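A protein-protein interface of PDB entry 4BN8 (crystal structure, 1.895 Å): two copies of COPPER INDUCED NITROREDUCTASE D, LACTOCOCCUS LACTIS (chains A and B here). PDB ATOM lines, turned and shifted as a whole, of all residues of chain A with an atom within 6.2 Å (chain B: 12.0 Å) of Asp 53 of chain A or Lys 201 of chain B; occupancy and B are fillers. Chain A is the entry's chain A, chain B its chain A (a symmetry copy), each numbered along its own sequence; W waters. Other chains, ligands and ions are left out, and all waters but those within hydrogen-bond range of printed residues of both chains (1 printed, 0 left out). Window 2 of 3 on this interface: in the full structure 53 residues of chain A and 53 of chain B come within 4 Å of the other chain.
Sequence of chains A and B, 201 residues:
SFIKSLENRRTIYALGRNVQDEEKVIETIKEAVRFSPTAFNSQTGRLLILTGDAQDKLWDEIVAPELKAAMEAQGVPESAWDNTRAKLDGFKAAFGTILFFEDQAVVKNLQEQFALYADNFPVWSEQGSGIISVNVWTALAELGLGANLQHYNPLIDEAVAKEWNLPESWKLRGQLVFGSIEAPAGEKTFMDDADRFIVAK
Water W1 lies within hydrogen-bond range of OG1 of Thr 51 of chain A (2.6 Å) and O of Ala 200 of chain B (2.9 Å).
CA of Val 199 of chain B touches O of Ile 49 of chain A (3.5 Å). CA of Leu 50 of chain A touches O of Ala 200 of chain B, 3.5 Å away. Thr 51 of chain A touches Lys 201 of chain B (O to C, 3.0 Å). N of Asp 53 of chain A touches C of Lys 201 of chain B, at 3.9 Å. Ala 54 of chain A touches Ala 200 of chain B. Ala 54 of chain A touches Lys 201 of chain B.
No position is printed for both chains. Of the 9 pairs that touch across the chains among the printed residues, none has its exchanged pair printed and touching as well.
N of Ile 49 of chain A is in hydrogen-bond range of O of Ile 198 of chain B. The backbone carbonyl oxygen of Ile 49 of chain A sits at hydrogen-bond distance from the backbone NH of Ala 200 of chain B. The backbone carbonyl oxygen (O) of Ala 200 of chain B sits at hydrogen-bond distance from the backbone NH (N) of Thr 51 of chain A.
Leu 50 of chain A touches one residue of chain B. No residue of chain B comes within 4 Å of Gly 52 of chain A. Of chain B, only Ala 200 (3.8 Å) and Lys 201 (3.5 Å) come within 4 Å of Ala 54 of chain A. Gln 55 of chain A touches none of the printed residues of chain B. No residue of chain B comes within 4 Å of Lys 57 of chain A. Leu 58 of chain A touches none of the printed residues of chain B. Of the printed residues of chain A, Val 199 of chain B touches Ile 49 (3.5 Å). Printed residues of chain A within 4 Å of Ala 200 of chain B: Ile 49, Leu 50, Thr 51 and Ala 54. Lys 201 of chain B touches just these residues of chain A: Thr 51 (3.0 Å), Asp 53 (3.9 Å) and Ala 54 (3.5 Å). The nearest residue of chain B that does not touch Asp 53 of chain A is Ala 200 of chain B (6.5 Å). The nearest residue of chain A that does not touch Lys 201 of chain B is Gly 52 of chain A (4.5 Å). The nearest printed residue of chain A that does not touch Ile 198 of chain B is Leu 50 of chain A (5.4 Å).
Of the 5 printed residues of chain B, 4 touch a printed residue of chain A. Printed residues of chain B that touch a printed residue of chain A: Ile 198, Val 199, Ala 200 and Lys 201. Hydrophobic or aromatic side chains of chain A within 4 Å of the printed part of chain B: Ile 49, Leu 50 and Ala 54. Among the printed residues, 9 pairs touch across the chains.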
ATOM      1  N   ILE A  49     -15.551 -29.948 -15.540  1.00  0.00           N
ATOM      2  CA  ILE A  49     -16.656 -30.691 -16.130  1.00  0.00           C
ATOM      3  C   ILE A  49     -17.966 -29.926 -15.904  1.00  0.00           C
ATOM      4  O   ILE A  49     -18.420 -29.764 -14.771  1.00  0.00           O
ATOM      5  CB  ILE A  49     -16.739 -32.104 -15.527  1.00  0.00           C
ATOM      6  CG1 ILE A  49     -15.411 -32.842 -15.739  1.00  0.00           C
ATOM      7  CG2 ILE A  49     -17.882 -32.892 -16.141  1.00  0.00           C
ATOM      8  CD1 ILE A  49     -15.276 -34.116 -14.909  1.00  0.00           C
ATOM      9  N   LEU A  50     -18.547 -29.432 -16.995  1.00  0.00           N
ATOM     10  CA  LEU A  50     -19.757 -28.617 -16.930  1.00  0.00           C
ATOM     11  C   LEU A  50     -20.963 -29.361 -17.486  1.00  0.00           C
ATOM     12  O   LEU A  50     -20.918 -29.897 -18.593  1.00  0.00           O
ATOM     13  CB  LEU A  50     -19.572 -27.328 -17.734  1.00  0.00           C
ATOM     14  CG  LEU A  50     -18.349 -26.467 -17.415  1.00  0.00           C
ATOM     15  CD1 LEU A  50     -18.404 -25.177 -18.217  1.00  0.00           C
ATOM     16  CD2 LEU A  50     -18.253 -26.175 -15.928  1.00  0.00           C
ATOM     17  N   THR A  51     -22.043 -29.380 -16.713  1.00  0.00           N
ATOM     18  CA  THR A  51     -23.323 -29.911 -17.172  1.00  0.00           C
ATOM     19  C   THR A  51     -24.446 -28.989 -16.712  1.00  0.00           C
ATOM     20  O   THR A  51     -24.213 -28.058 -15.941  1.00  0.00           O
ATOM     21  CB  THR A  51     -23.592 -31.330 -16.621  1.00  0.00           C
ATOM     22  OG1 THR A  51     -23.850 -31.257 -15.214  1.00  0.00           O
ATOM     23  CG2 THR A  51     -22.406 -32.246 -16.876  1.00  0.00           C
ATOM     24  N   GLY A  52     -25.662 -29.245 -17.180  1.00  0.00           N
ATOM     25  CA  GLY A  52     -26.816 -28.463 -16.758  1.00  0.00           C
ATOM     26  C   GLY A  52     -26.649 -26.969 -16.976  1.00  0.00           C
ATOM     27  O   GLY A  52     -26.242 -26.536 -18.048  1.00  0.00           O
ATOM     28  N   ASP A  53     -26.962 -26.175 -15.955  1.00  0.00           N
ATOM     29  CA  ASP A  53     -26.924 -24.718 -16.073  1.00  0.00           C
ATOM     30  C   ASP A  53     -25.543 -24.213 -16.491  1.00  0.00           C
ATOM     31  O   ASP A  53     -25.425 -23.215 -17.203  1.00  0.00           O
ATOM     32  CB  ASP A  53     -27.324 -24.063 -14.747  1.00  0.00           C
ATOM     33  CG  ASP A  53     -28.797 -24.239 -14.429  1.00  0.00           C
ATOM     34  OD1 ASP A  53     -29.591 -24.456 -15.369  1.00  0.00           O
ATOM     35  OD2 ASP A  53     -29.166 -24.149 -13.239  1.00  0.00           O
ATOM     36  N   ALA A  54     -24.501 -24.906 -16.041  1.00  0.00           N
ATOM     37  CA  ALA A  54     -23.127 -24.506 -16.332  1.00  0.00           C
ATOM     38  C   ALA A  54     -22.818 -24.706 -17.812  1.00  0.00           C
ATOM     39  O   ALA A  54     -22.127 -23.895 -18.431  1.00  0.00           O
ATOM     40  CB  ALA A  54     -22.150 -25.289 -15.468  1.00  0.00           C
ATOM     41  N   GLN A  55     -23.331 -25.795 -18.369  1.00  0.00           N
ATOM     42  CA  GLN A  55     -23.217 -26.056 -19.795  1.00  0.00           C
ATOM     43  C   GLN A  55     -23.869 -24.908 -20.574  1.00  0.00           C
ATOM     44  O   GLN A  55     -23.298 -24.398 -21.535  1.00  0.00           O
ATOM     45  CB  GLN A  55     -23.872 -27.402 -20.121  1.00  0.00           C
ATOM     46  CG  GLN A  55     -24.228 -27.625 -21.580  1.00  0.00           C
ATOM     47  CD  GLN A  55     -23.015 -27.833 -22.460  1.00  0.00           C
ATOM     48  OE1 GLN A  55     -21.879 -27.824 -21.988  1.00  0.00           O
ATOM     49  NE2 GLN A  55     -23.253 -28.021 -23.749  1.00  0.00           N
ATOM     50  N   ASP A  56     -25.058 -24.491 -20.145  1.00  0.00           N
ATOM     51  CA  ASP A  56     -25.760 -23.386 -20.803  1.00  0.00           C
ATOM     52  C   ASP A  56     -24.963 -22.086 -20.696  1.00  0.00           C
ATOM     53  O   ASP A  56     -24.807 -21.358 -21.676  1.00  0.00           O
ATOM     54  CB  ASP A  56     -27.155 -23.183 -20.199  1.00  0.00           C
ATOM     55  CG  ASP A  56     -28.108 -24.316 -20.529  1.00  0.00           C
ATOM     56  OD1 ASP A  56     -27.844 -25.060 -21.495  1.00  0.00           O
ATOM     57  OD2 ASP A  56     -29.129 -24.457 -19.822  1.00  0.00           O
ATOM     58  N   LYS A  57     -24.463 -21.802 -19.501  1.00  0.00           N
ATOM     59  CA  LYS A  57     -23.692 -20.589 -19.263  1.00  0.00           C
ATOM     60  C   LYS A  57     -22.453 -20.520 -20.150  1.00  0.00           C
ATOM     61  O   LYS A  57     -22.174 -19.485 -20.752  1.00  0.00           O
ATOM     62  CB  LYS A  57     -23.285 -20.494 -17.792  1.00  0.00           C
ATOM     63  CG  LYS A  57     -22.497 -19.240 -17.463  1.00  0.00           C
ATOM     64  CD  LYS A  57     -22.275 -19.085 -15.972  1.00  0.00           C
ATOM     65  CE  LYS A  57     -23.574 -18.792 -15.239  1.00  0.00           C
ATOM     66  NZ  LYS A  57     -23.332 -18.276 -13.863  1.00  0.00           N
ATOM     67  N   LEU A  58     -21.710 -21.615 -20.237  1.00  0.00           N
ATOM     68  CA  LEU A  58     -20.495 -21.622 -21.040  1.00  0.00           C
ATOM     69  C   LEU A  58     -20.768 -21.128 -22.458  1.00  0.00           C
ATOM     70  O   LEU A  58     -20.092 -20.231 -22.955  1.00  0.00           O
ATOM     71  CB  LEU A  58     -19.887 -23.023 -21.100  1.00  0.00           C
ATOM     72  CG  LEU A  58     -18.699 -23.137 -22.061  1.00  0.00           C
ATOM     73  CD1 LEU A  58     -17.578 -22.210 -21.635  1.00  0.00           C
ATOM     74  CD2 LEU A  58     -18.197 -24.572 -22.164  1.00  0.00           C
ATOM     75  N   PHE B 197      -9.864 -32.405 -10.696  1.00  0.00           N
ATOM     76  CA  PHE B 197     -11.201 -32.441 -11.283  1.00  0.00           C
ATOM     77  C   PHE B 197     -12.140 -31.471 -10.570  1.00  0.00           C
ATOM     78  O   PHE B 197     -12.303 -31.540  -9.352  1.00  0.00           O
ATOM     79  CB  PHE B 197     -11.803 -33.848 -11.213  1.00  0.00           C
ATOM     80  CG  PHE B 197     -10.916 -34.928 -11.772  1.00  0.00           C
ATOM     81  CD1 PHE B 197     -10.698 -35.031 -13.136  1.00  0.00           C
ATOM     82  CD2 PHE B 197     -10.330 -35.862 -10.931  1.00  0.00           C
ATOM     83  CE1 PHE B 197      -9.897 -36.036 -13.649  1.00  0.00           C
ATOM     84  CE2 PHE B 197      -9.524 -36.863 -11.431  1.00  0.00           C
ATOM     85  CZ  PHE B 197      -9.305 -36.954 -12.791  1.00  0.00           C
ATOM     86  N   ILE B 198     -12.746 -30.570 -11.341  1.00  0.00           N
ATOM     87  CA  ILE B 198     -13.820 -29.714 -10.849  1.00  0.00           C
ATOM     88  C   ILE B 198     -15.091 -30.030 -11.622  1.00  0.00           C
ATOM     89  O   ILE B 198     -15.102 -30.001 -12.851  1.00  0.00           O
ATOM     90  CB  ILE B 198     -13.503 -28.221 -11.035  1.00  0.00           C
ATOM     91  CG1 ILE B 198     -12.277 -27.826 -10.212  1.00  0.00           C
ATOM     92  CG2 ILE B 198     -14.706 -27.360 -10.616  1.00  0.00           C
ATOM     93  CD1 ILE B 198     -11.796 -26.412 -10.465  1.00  0.00           C
ATOM     94  N   VAL B 199     -16.158 -30.339 -10.895  1.00  0.00           N
ATOM     95  CA  VAL B 199     -17.446 -30.620 -11.507  1.00  0.00           C
ATOM     96  C   VAL B 199     -18.429 -29.532 -11.104  1.00  0.00           C
ATOM     97  O   VAL B 199     -18.592 -29.243  -9.920  1.00  0.00           O
ATOM     98  CB  VAL B 199     -17.988 -31.990 -11.066  1.00  0.00           C
ATOM     99  CG1 VAL B 199     -19.331 -32.265 -11.716  1.00  0.00           C
ATOM    100  CG2 VAL B 199     -16.991 -33.086 -11.393  1.00  0.00           C
ATOM    101  N   ALA B 200     -19.073 -28.924 -12.093  1.00  0.00           N
ATOM    102  CA  ALA B 200     -20.045 -27.869 -11.846  1.00  0.00           C
ATOM    103  C   ALA B 200     -21.343 -28.144 -12.600  1.00  0.00           C
ATOM    104  O   ALA B 200     -21.329 -28.551 -13.766  1.00  0.00           O
ATOM    105  CB  ALA B 200     -19.472 -26.519 -12.251  1.00  0.00           C
ATOM    106  N   LYS B 201     -22.465 -27.923 -11.924  1.00  0.00           N
ATOM    107  CA  LYS B 201     -23.783 -28.172 -12.500  1.00  0.00           C
ATOM    108  C   LYS B 201     -24.322 -26.918 -13.178  1.00  0.00           C
ATOM    109  O   LYS B 201     -24.650 -25.933 -12.515  1.00  0.00           O
ATOM    110  CB  LYS B 201     -24.747 -28.645 -11.417  1.00  0.00           C
HETATM  111  O   HOH W   1     -21.714 -31.379 -13.661  1.00  0.00           O
